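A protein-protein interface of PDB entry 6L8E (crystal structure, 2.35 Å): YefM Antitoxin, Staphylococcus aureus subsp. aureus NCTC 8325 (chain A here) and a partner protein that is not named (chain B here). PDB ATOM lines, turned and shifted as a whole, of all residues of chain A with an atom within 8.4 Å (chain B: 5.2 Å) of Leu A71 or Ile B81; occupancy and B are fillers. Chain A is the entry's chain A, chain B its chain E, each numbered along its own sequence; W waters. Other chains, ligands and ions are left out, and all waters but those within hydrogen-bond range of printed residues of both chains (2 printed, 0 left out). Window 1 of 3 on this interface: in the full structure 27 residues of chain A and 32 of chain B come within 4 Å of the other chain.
O of Ile A77 is in hydrogen-bond range of N of Phe B8. The side-chain hydroxyl of Ser A67 lies close to the backbone carbonyl oxygen of Ala B82, at 3.4 Å. The backbone carbonyl oxygen of Lys A79 sits at hydrogen-bond distance from the backbone NH of Ile B6 (2.9 Å). The side-chain hydroxyl (OG) of Ser B83 is in hydrogen-bond range of a ring nitrogen (NE2) of His A63 (2.8 Å).
OG of Ser A67 lies within hydrogen-bond range of O of His A63. The backbone NH (N) of Val B71 is in hydrogen-bond range of the backbone carbonyl oxygen (O) of Ser B83 (2.8 Å). The side-chain hydroxyl (OG) of Ser B9 is in hydrogen-bond range of the backbone NH (N) of Ala B12. N of Ile B81 sits at hydrogen-bond distance from O of Thr B7. N of Thr B7 is in hydrogen-bond range of O of Ile B79 (3.0 Å). N of Ala B82 sits at hydrogen-bond distance from O of Val B71, 2.7 Å away.
Among the printed residues, pairs that only touch across the chains: Leu A64 with Ser B83, Ser A67 with Ser B9, Ile A68 with Tyr B59, Leu A71 with Thr B7, Leu A71 with Phe B8, Leu A71 with Ser B9, Leu A71 with Tyr B59, Leu A71 with Ile B81, Leu A71 with Ala B82, Thr A76 with Thr B7, Thr A76 with Phe B8, Ile A77 with Ile B6, Ile A77 with Thr B7, Lys A79 with Phe B8, Ile A81 with Phe B8 and Ile A81 with Leu B34.
Of chain B, only Thr B7 (3.7 Å), Phe B8 (3.9 Å), Ser B9 (3.7 Å), Tyr B59 (3.4 Å), Ile B81 (3.8 Å) and Ala B82 (3.8 Å) come within 4 Å of Leu A71. Ile B81 touches just one residue of chain A: Leu A71. Of the printed residues of chain A, Ile B6 touches Ile A77 (3.8 Å) and Lys A79 (2.9 Å). Printed residues of chain B within 4 Å of Ile A68: Tyr B59. Of the printed residues of chain B, Thr A76 touches Thr B7 (3.6 Å) and Phe B8 (3.5 Å). Printed residues of chain B within 4 Å of Ile A77: Ile B6 (3.8 Å), Thr B7 (3.7 Å) and Phe B8 (2.8 Å). Printed residues of chain B within 4 Å of Ser A67: Ser B9 (3.5 Å) and Ala B82 (3.2 Å). The nearest residue of chain B that does not touch Leu A71 is Lys B80 (4.2 Å).
Of the 17 printed residues of chain A, 9 touch a printed residue of chain B. Hydrophobic or aromatic side chains of chain A within 4 Å of the printed part of chain B: His A63, Leu A64, Ile A68, Leu A71 and Ile A81. Of the 16 printed residues of chain B, 9 touch a printed residue of chain A. Among the printed residues, 20 pairs touch across the chains.
Water W2 lies within hydrogen-bond range of the backbone carbonyl oxygen of Leu A71 (2.5 Å) and the side-chain amino group of Lys B80 (2.7 Å). Water W1 lies within hydrogen-bond range of the backbone NH of Cys B84 (3.0 Å), the side-chain hydroxyl of Ser B83 (3.0 Å) and a ring nitrogen (NE2) of His A63 (3.3 Å).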
ATOM      1  N   HIS A  63       8.506  16.590   7.307  1.00  0.00           N
ATOM      2  CA  HIS A  63       8.272  16.588   5.867  1.00  0.00           C
ATOM      3  C   HIS A  63       9.297  17.451   5.143  1.00  0.00           C
ATOM      4  O   HIS A  63       9.833  17.055   4.101  1.00  0.00           O
ATOM      5  CB  HIS A  63       6.851  17.074   5.576  1.00  0.00           C
ATOM      6  CG  HIS A  63       6.698  17.737   4.242  1.00  0.00           C
ATOM      7  ND1 HIS A  63       6.762  17.043   3.053  1.00  0.00           N
ATOM      8  CD2 HIS A  63       6.481  19.033   3.911  1.00  0.00           C
ATOM      9  CE1 HIS A  63       6.592  17.884   2.048  1.00  0.00           C
ATOM     10  NE2 HIS A  63       6.419  19.096   2.541  1.00  0.00           N
ATOM     11  N   LEU A  64       9.591  18.632   5.692  1.00  0.00           N
ATOM     12  CA  LEU A  64      10.573  19.524   5.086  1.00  0.00           C
ATOM     13  C   LEU A  64      11.986  18.961   5.198  1.00  0.00           C
ATOM     14  O   LEU A  64      12.753  19.006   4.232  1.00  0.00           O
ATOM     15  CB  LEU A  64      10.486  20.906   5.732  1.00  0.00           C
ATOM     16  CG  LEU A  64       9.244  21.720   5.379  1.00  0.00           C
ATOM     17  CD1 LEU A  64       9.277  23.060   6.084  1.00  0.00           C
ATOM     18  CD2 LEU A  64       9.173  21.908   3.881  1.00  0.00           C
ATOM     19  N   ALA A  65      12.346  18.426   6.370  1.00  0.00           N
ATOM     20  CA  ALA A  65      13.668  17.829   6.553  1.00  0.00           C
ATOM     21  C   ALA A  65      13.896  16.683   5.572  1.00  0.00           C
ATOM     22  O   ALA A  65      14.953  16.598   4.937  1.00  0.00           O
ATOM     23  CB  ALA A  65      13.839  17.351   7.994  1.00  0.00           C
ATOM     24  N   GLN A  66      12.902  15.803   5.423  1.00  0.00           N
ATOM     25  CA  GLN A  66      13.033  14.657   4.528  1.00  0.00           C
ATOM     26  C   GLN A  66      13.075  15.094   3.068  1.00  0.00           C
ATOM     27  O   GLN A  66      13.840  14.540   2.269  1.00  0.00           O
ATOM     28  CB  GLN A  66      11.888  13.675   4.769  1.00  0.00           C
ATOM     29  CG  GLN A  66      11.975  12.387   3.955  1.00  0.00           C
ATOM     30  CD  GLN A  66      13.284  11.649   4.175  1.00  0.00           C
ATOM     31  OE1 GLN A  66      13.626  11.297   5.305  1.00  0.00           O
ATOM     32  NE2 GLN A  66      14.033  11.425   3.097  1.00  0.00           N
ATOM     33  N   SER A  67      12.271  16.095   2.702  1.00  0.00           N
ATOM     34  CA  SER A  67      12.224  16.528   1.310  1.00  0.00           C
ATOM     35  C   SER A  67      13.514  17.224   0.908  1.00  0.00           C
ATOM     36  O   SER A  67      14.025  17.005  -0.196  1.00  0.00           O
ATOM     37  CB  SER A  67      11.031  17.448   1.076  1.00  0.00           C
ATOM     38  OG  SER A  67       9.818  16.797   1.399  1.00  0.00           O
ATOM     39  N   ILE A  68      14.051  18.068   1.790  1.00  0.00           N
ATOM     40  CA  ILE A  68      15.325  18.721   1.511  1.00  0.00           C
ATOM     41  C   ILE A  68      16.439  17.687   1.414  1.00  0.00           C
ATOM     42  O   ILE A  68      17.326  17.789   0.560  1.00  0.00           O
ATOM     43  CB  ILE A  68      15.625  19.787   2.581  1.00  0.00           C
ATOM     44  CG1 ILE A  68      14.656  20.964   2.441  1.00  0.00           C
ATOM     45  CG2 ILE A  68      17.068  20.259   2.474  1.00  0.00           C
ATOM     46  CD1 ILE A  68      14.742  21.948   3.566  1.00  0.00           C
ATOM     47  N   ALA A  69      16.394  16.664   2.273  1.00  0.00           N
ATOM     48  CA  ALA A  69      17.382  15.590   2.207  1.00  0.00           C
ATOM     49  C   ALA A  69      17.288  14.841   0.883  1.00  0.00           C
ATOM     50  O   ALA A  69      18.313  14.521   0.269  1.00  0.00           O
ATOM     51  CB  ALA A  69      17.200  14.631   3.382  1.00  0.00           C
ATOM     52  N   ASP A  70      16.066  14.557   0.427  1.00  0.00           N
ATOM     53  CA  ASP A  70      15.885  13.903  -0.864  1.00  0.00           C
ATOM     54  C   ASP A  70      16.503  14.727  -1.986  1.00  0.00           C
ATOM     55  O   ASP A  70      17.225  14.197  -2.839  1.00  0.00           O
ATOM     56  CB  ASP A  70      14.401  13.670  -1.133  1.00  0.00           C
ATOM     57  CG  ASP A  70      13.819  12.591  -0.260  1.00  0.00           C
ATOM     58  OD1 ASP A  70      14.605  11.764   0.253  1.00  0.00           O
ATOM     59  OD2 ASP A  70      12.582  12.567  -0.090  1.00  0.00           O
ATOM     60  N   LEU A  71      16.223  16.032  -2.000  1.00  0.00           N
ATOM     61  CA  LEU A  71      16.774  16.901  -3.032  1.00  0.00           C
ATOM     62  C   LEU A  71      18.295  16.915  -2.990  1.00  0.00           C
ATOM     63  O   LEU A  71      18.952  16.969  -4.036  1.00  0.00           O
ATOM     64  CB  LEU A  71      16.224  18.319  -2.871  1.00  0.00           C
ATOM     65  CG  LEU A  71      14.740  18.528  -3.173  1.00  0.00           C
ATOM     66  CD1 LEU A  71      14.321  19.945  -2.818  1.00  0.00           C
ATOM     67  CD2 LEU A  71      14.461  18.237  -4.637  1.00  0.00           C
ATOM     68  N   GLU A  72      18.873  16.856  -1.790  1.00  0.00           N
ATOM     69  CA  GLU A  72      20.323  16.929  -1.664  1.00  0.00           C
ATOM     70  C   GLU A  72      20.994  15.589  -1.925  1.00  0.00           C
ATOM     71  O   GLU A  72      22.195  15.560  -2.209  1.00  0.00           O
ATOM     72  CB  GLU A  72      20.700  17.469  -0.282  1.00  0.00           C
ATOM     73  CG  GLU A  72      20.238  18.914  -0.090  1.00  0.00           C
ATOM     74  CD  GLU A  72      20.511  19.475   1.294  1.00  0.00           C
ATOM     75  OE1 GLU A  72      20.840  18.690   2.207  1.00  0.00           O
ATOM     76  OE2 GLU A  72      20.394  20.711   1.464  1.00  0.00           O
ATOM     77  N   ARG A  73      20.244  14.490  -1.870  1.00  0.00           N
ATOM     78  CA  ARG A  73      20.736  13.173  -2.245  1.00  0.00           C
ATOM     79  C   ARG A  73      20.293  12.761  -3.646  1.00  0.00           C
ATOM     80  O   ARG A  73      20.495  11.607  -4.036  1.00  0.00           O
ATOM     81  CB  ARG A  73      20.288  12.131  -1.218  1.00  0.00           C
ATOM     82  CG  ARG A  73      20.745  12.452   0.199  1.00  0.00           C
ATOM     83  CD  ARG A  73      20.386  11.352   1.186  1.00  0.00           C
ATOM     84  NE  ARG A  73      21.114  11.507   2.445  1.00  0.00           N
ATOM     85  CZ  ARG A  73      20.543  11.609   3.643  1.00  0.00           C
ATOM     86  NH1 ARG A  73      21.294  11.750   4.726  1.00  0.00           N
ATOM     87  NH2 ARG A  73      19.224  11.555   3.761  1.00  0.00           N
ATOM     88  N   GLY A  74      19.698  13.674  -4.408  1.00  0.00           N
ATOM     89  CA  GLY A  74      19.405  13.393  -5.797  1.00  0.00           C
ATOM     90  C   GLY A  74      18.184  12.539  -6.045  1.00  0.00           C
ATOM     91  O   GLY A  74      17.958  12.121  -7.186  1.00  0.00           O
ATOM     92  N   LYS A  75      17.388  12.260  -5.008  1.00  0.00           N
ATOM     93  CA  LYS A  75      16.124  11.536  -5.152  1.00  0.00           C
ATOM     94  C   LYS A  75      15.041  12.546  -5.502  1.00  0.00           C
ATOM     95  O   LYS A  75      14.423  13.141  -4.618  1.00  0.00           O
ATOM     96  CB  LYS A  75      15.781  10.773  -3.880  1.00  0.00           C
ATOM     97  CG  LYS A  75      14.653   9.770  -4.076  1.00  0.00           C
ATOM     98  CD  LYS A  75      14.344   8.989  -2.811  1.00  0.00           C
ATOM     99  CE  LYS A  75      13.374   7.848  -3.092  1.00  0.00           C
ATOM    100  NZ  LYS A  75      12.117   7.963  -2.301  1.00  0.00           N
ATOM    101  N   THR A  76      14.808  12.749  -6.797  1.00  0.00           N
ATOM    102  CA  THR A  76      13.954  13.834  -7.255  1.00  0.00           C
ATOM    103  C   THR A  76      13.039  13.371  -8.379  1.00  0.00           C
ATOM    104  O   THR A  76      13.181  12.276  -8.929  1.00  0.00           O
ATOM    105  CB  THR A  76      14.773  15.027  -7.761  1.00  0.00           C
ATOM    106  OG1 THR A  76      15.436  14.657  -8.977  1.00  0.00           O
ATOM    107  CG2 THR A  76      15.811  15.454  -6.735  1.00  0.00           C
ATOM    108  N   ILE A  77      12.093  14.245  -8.722  1.00  0.00           N
ATOM    109  CA  ILE A  77      11.208  14.080  -9.868  1.00  0.00           C
ATOM    110  C   ILE A  77      11.247  15.373 -10.671  1.00  0.00           C
ATOM    111  O   ILE A  77      11.109  16.462 -10.102  1.00  0.00           O
ATOM    112  CB  ILE A  77       9.760  13.766  -9.442  1.00  0.00           C
ATOM    113  CG1 ILE A  77       9.715  12.591  -8.460  1.00  0.00           C
ATOM    114  CG2 ILE A  77       8.890  13.499 -10.668  1.00  0.00           C
ATOM    115  CD1 ILE A  77      10.036  11.249  -9.078  1.00  0.00           C
ATOM    116  N   LYS A  79       9.506  17.829 -13.408  1.00  0.00           N
ATOM    117  CA  LYS A  79       8.306  18.210 -14.128  1.00  0.00           C
ATOM    118  C   LYS A  79       8.632  19.352 -15.076  1.00  0.00           C
ATOM    119  O   LYS A  79       9.479  20.199 -14.783  1.00  0.00           O
ATOM    120  CB  LYS A  79       7.179  18.634 -13.181  1.00  0.00           C
ATOM    121  CG  LYS A  79       6.512  17.478 -12.469  1.00  0.00           C
ATOM    122  CD  LYS A  79       5.168  17.886 -11.895  1.00  0.00           C
ATOM    123  CE  LYS A  79       4.249  18.433 -12.986  1.00  0.00           C
ATOM    124  NZ  LYS A  79       3.923  17.390 -14.006  1.00  0.00           N
ATOM    125  N   ILE A  81       6.624  22.462 -16.737  1.00  0.00           N
ATOM    126  CA  ILE A  81       5.421  23.206 -16.392  1.00  0.00           C
ATOM    127  C   ILE A  81       5.310  24.410 -17.313  1.00  0.00           C
ATOM    128  O   ILE A  81       6.222  25.244 -17.365  1.00  0.00           O
ATOM    129  CB  ILE A  81       5.427  23.642 -14.921  1.00  0.00           C
ATOM    130  CG1 ILE A  81       5.292  22.413 -14.021  1.00  0.00           C
ATOM    131  CG2 ILE A  81       4.307  24.629 -14.645  1.00  0.00           C
ATOM    132  CD1 ILE A  81       5.506  22.695 -12.558  1.00  0.00           C
ATOM    133  N   ILE B   6      11.457  21.981 -13.722  1.00  0.00           N
ATOM    134  CA  ILE B   6      11.393  22.144 -12.273  1.00  0.00           C
ATOM    135  C   ILE B   6      11.723  20.819 -11.599  1.00  0.00           C
ATOM    136  O   ILE B   6      11.203  19.770 -11.995  1.00  0.00           O
ATOM    137  CB  ILE B   6      10.005  22.635 -11.821  1.00  0.00           C
ATOM    138  CG1 ILE B   6       9.596  23.889 -12.597  1.00  0.00           C
ATOM    139  CG2 ILE B   6       9.987  22.895 -10.325  1.00  0.00           C
ATOM    140  CD1 ILE B   6      10.474  25.086 -12.327  1.00  0.00           C
ATOM    141  N   THR B   7      12.566  20.868 -10.571  1.00  0.00           N
ATOM    142  CA  THR B   7      12.840  19.697  -9.749  1.00  0.00           C
ATOM    143  C   THR B   7      11.912  19.699  -8.545  1.00  0.00           C
ATOM    144  O   THR B   7      11.770  20.719  -7.862  1.00  0.00           O
ATOM    145  CB  THR B   7      14.299  19.679  -9.288  1.00  0.00           C
ATOM    146  OG1 THR B   7      15.147  19.448 -10.416  1.00  0.00           O
ATOM    147  CG2 THR B   7      14.532  18.582  -8.272  1.00  0.00           C
ATOM    148  N   PHE B   8      11.265  18.564  -8.298  1.00  0.00           N
ATOM    149  CA  PHE B   8      10.424  18.370  -7.126  1.00  0.00           C
ATOM    150  C   PHE B   8      11.048  17.316  -6.230  1.00  0.00           C
ATOM    151  O   PHE B   8      11.647  16.352  -6.717  1.00  0.00           O
ATOM    152  CB  PHE B   8       9.006  17.907  -7.494  1.00  0.00           C
ATOM    153  CG  PHE B   8       8.142  18.976  -8.084  1.00  0.00           C
ATOM    154  CD1 PHE B   8       8.303  19.370  -9.404  1.00  0.00           C
ATOM    155  CD2 PHE B   8       7.144  19.568  -7.327  1.00  0.00           C
ATOM    156  CE1 PHE B   8       7.493  20.349  -9.949  1.00  0.00           C
ATOM    157  CE2 PHE B   8       6.336  20.549  -7.865  1.00  0.00           C
ATOM    158  CZ  PHE B   8       6.510  20.942  -9.176  1.00  0.00           C
ATOM    159  N   SER B   9      10.894  17.500  -4.920  1.00  0.00           N
ATOM    160  CA  SER B   9      11.096  16.399  -4.002  1.00  0.00           C
ATOM    161  C   SER B   9       9.982  15.377  -4.220  1.00  0.00           C
ATOM    162  O   SER B   9       8.928  15.714  -4.768  1.00  0.00           O
ATOM    163  CB  SER B   9      11.097  16.902  -2.558  1.00  0.00           C
ATOM    164  OG  SER B   9       9.802  17.323  -2.153  1.00  0.00           O
ATOM    165  N   ALA B  12       6.773  16.630  -2.463  1.00  0.00           N
ATOM    166  CA  ALA B  12       6.188  17.794  -3.118  1.00  0.00           C
ATOM    167  C   ALA B  12       5.571  17.424  -4.461  1.00  0.00           C
ATOM    168  O   ALA B  12       4.589  18.044  -4.883  1.00  0.00           O
ATOM    169  CB  ALA B  12       7.241  18.886  -3.299  1.00  0.00           C
ATOM    170  N   LEU B  34       6.152  30.227  -9.511  1.00  0.00           N
ATOM    171  CA  LEU B  34       7.307  29.706 -10.235  1.00  0.00           C
ATOM    172  C   LEU B  34       7.752  30.672 -11.327  1.00  0.00           C
ATOM    173  O   LEU B  34       8.953  30.918 -11.495  1.00  0.00           O
ATOM    174  CB  LEU B  34       6.983  28.329 -10.822  1.00  0.00           C
ATOM    175  CG  LEU B  34       6.804  27.216  -9.790  1.00  0.00           C
ATOM    176  CD1 LEU B  34       6.322  25.924 -10.429  1.00  0.00           C
ATOM    177  CD2 LEU B  34       8.113  26.996  -9.052  1.00  0.00           C
ATOM    178  N   TYR B  59      17.001  27.626   1.686  1.00  0.00           N
ATOM    179  CA  TYR B  59      15.710  27.546   1.028  1.00  0.00           C
ATOM    180  C   TYR B  59      14.881  28.787   1.317  1.00  0.00           C
ATOM    181  O   TYR B  59      15.151  29.550   2.248  1.00  0.00           O
ATOM    182  CB  TYR B  59      14.954  26.285   1.456  1.00  0.00           C
ATOM    183  CG  TYR B  59      15.428  25.065   0.708  1.00  0.00           C
ATOM    184  CD1 TYR B  59      16.629  24.455   1.040  1.00  0.00           C
ATOM    185  CD2 TYR B  59      14.696  24.542  -0.352  1.00  0.00           C
ATOM    186  CE1 TYR B  59      17.086  23.353   0.356  1.00  0.00           C
ATOM    187  CE2 TYR B  59      15.146  23.434  -1.046  1.00  0.00           C
ATOM    188  CZ  TYR B  59      16.346  22.844  -0.681  1.00  0.00           C
ATOM    189  OH  TYR B  59      16.820  21.741  -1.351  1.00  0.00           O
ATOM    190  N   LEU B  70       5.091  27.520  -0.700  1.00  0.00           N
ATOM    191  CA  LEU B  70       6.001  26.953  -1.686  1.00  0.00           C
ATOM    192  C   LEU B  70       7.418  27.101  -1.148  1.00  0.00           C
ATOM    193  O   LEU B  70       7.971  28.203  -1.145  1.00  0.00           O
ATOM    194  CB  LEU B  70       5.858  27.656  -3.031  1.00  0.00           C
ATOM    195  CG  LEU B  70       6.716  27.130  -4.181  1.00  0.00           C
ATOM    196  CD1 LEU B  70       6.278  25.736  -4.621  1.00  0.00           C
ATOM    197  CD2 LEU B  70       6.660  28.098  -5.346  1.00  0.00           C
ATOM    198  N   VAL B  71       7.998  25.999  -0.683  1.00  0.00           N
ATOM    199  CA  VAL B  71       9.353  25.986  -0.146  1.00  0.00           C
ATOM    200  C   VAL B  71      10.290  25.516  -1.247  1.00  0.00           C
ATOM    201  O   VAL B  71      10.156  24.395  -1.753  1.00  0.00           O
ATOM    202  CB  VAL B  71       9.452  25.088   1.094  1.00  0.00           C
ATOM    203  CG1 VAL B  71      10.851  25.151   1.663  1.00  0.00           C
ATOM    204  CG2 VAL B  71       8.427  25.517   2.131  1.00  0.00           C
ATOM    205  N   TYR B  72      11.244  26.368  -1.614  1.00  0.00           N
ATOM    206  CA  TYR B  72      12.027  26.159  -2.822  1.00  0.00           C
ATOM    207  C   TYR B  72      13.441  26.684  -2.624  1.00  0.00           C
ATOM    208  O   TYR B  72      13.745  27.379  -1.651  1.00  0.00           O
ATOM    209  CB  TYR B  72      11.368  26.852  -4.023  1.00  0.00           C
ATOM    210  CG  TYR B  72      11.321  28.356  -3.873  1.00  0.00           C
ATOM    211  CD1 TYR B  72      10.278  28.980  -3.194  1.00  0.00           C
ATOM    212  CD2 TYR B  72      12.327  29.152  -4.404  1.00  0.00           C
ATOM    213  CE1 TYR B  72      10.240  30.352  -3.051  1.00  0.00           C
ATOM    214  CE2 TYR B  72      12.296  30.524  -4.268  1.00  0.00           C
ATOM    215  CZ  TYR B  72      11.248  31.119  -3.590  1.00  0.00           C
ATOM    216  OH  TYR B  72      11.200  32.486  -3.443  1.00  0.00           O
ATOM    217  N   ILE B  79      15.096  25.792 -10.518  1.00  0.00           N
ATOM    218  CA  ILE B  79      14.246  25.818  -9.334  1.00  0.00           C
ATOM    219  C   ILE B  79      14.039  24.394  -8.834  1.00  0.00           C
ATOM    220  O   ILE B  79      13.772  23.476  -9.622  1.00  0.00           O
ATOM    221  CB  ILE B  79      12.899  26.488  -9.649  1.00  0.00           C
ATOM    222  CG1 ILE B  79      13.114  27.885 -10.238  1.00  0.00           C
ATOM    223  CG2 ILE B  79      12.028  26.552  -8.412  1.00  0.00           C
ATOM    224  CD1 ILE B  79      11.834  28.554 -10.722  1.00  0.00           C
ATOM    225  N   LYS B  80      14.156  24.204  -7.524  1.00  0.00           N
ATOM    226  CA  LYS B  80      13.815  22.945  -6.876  1.00  0.00           C
ATOM    227  C   LYS B  80      12.730  23.205  -5.846  1.00  0.00           C
ATOM    228  O   LYS B  80      12.830  24.159  -5.071  1.00  0.00           O
ATOM    229  CB  LYS B  80      15.022  22.315  -6.178  1.00  0.00           C
ATOM    230  CG  LYS B  80      16.312  22.272  -6.967  1.00  0.00           C
ATOM    231  CD  LYS B  80      17.333  21.439  -6.203  1.00  0.00           C
ATOM    232  CE  LYS B  80      18.728  21.547  -6.784  1.00  0.00           C
ATOM    233  NZ  LYS B  80      19.617  20.502  -6.199  1.00  0.00           N
ATOM    234  N   ILE B  81      11.719  22.345  -5.815  1.00  0.00           N
ATOM    235  CA  ILE B  81      10.609  22.479  -4.878  1.00  0.00           C
ATOM    236  C   ILE B  81      10.770  21.434  -3.784  1.00  0.00           C
ATOM    237  O   ILE B  81      10.775  20.228  -4.056  1.00  0.00           O
ATOM    238  CB  ILE B  81       9.249  22.337  -5.578  1.00  0.00           C
ATOM    239  CG1 ILE B  81       9.157  23.273  -6.790  1.00  0.00           C
ATOM    240  CG2 ILE B  81       8.118  22.591  -4.586  1.00  0.00           C
ATOM    241  CD1 ILE B  81       9.416  24.733  -6.478  1.00  0.00           C
ATOM    242  N   ALA B  82      10.915  21.897  -2.544  1.00  0.00           N
ATOM    243  CA  ALA B  82      10.907  20.981  -1.413  1.00  0.00           C
ATOM    244  C   ALA B  82       9.492  20.705  -0.933  1.00  0.00           C
ATOM    245  O   ALA B  82       9.204  19.594  -0.477  1.00  0.00           O
ATOM    246  CB  ALA B  82      11.755  21.541  -0.267  1.00  0.00           C
ATOM    247  N   SER B  83       8.599  21.687  -1.048  1.00  0.00           N
ATOM    248  CA  SER B  83       7.243  21.575  -0.532  1.00  0.00           C
ATOM    249  C   SER B  83       6.336  22.558  -1.258  1.00  0.00           C
ATOM    250  O   SER B  83       6.761  23.651  -1.641  1.00  0.00           O
ATOM    251  CB  SER B  83       7.199  21.840   0.973  1.00  0.00           C
ATOM    252  OG  SER B  83       5.888  21.665   1.488  1.00  0.00           O
ATOM    253  N   CYS B  84       5.072  22.158  -1.426  1.00  0.00           N
ATOM    254  CA  CYS B  84       4.059  23.053  -1.970  1.00  0.00           C
ATOM    255  C   CYS B  84       2.717  22.857  -1.269  1.00  0.00           C
ATOM    256  O   CYS B  84       1.672  23.184  -1.846  1.00  0.00           O
ATOM    257  CB  CYS B  84       3.904  22.853  -3.484  1.00  0.00           C
ATOM    258  SG  CYS B  84       3.219  21.248  -3.970  1.00  0.00           S
HETATM  259  O   HOH W   1       4.676  19.507  -0.186  1.00  0.00           O
HETATM  260  O   HOH W   2      18.611  17.976  -6.348  1.00  0.00           O
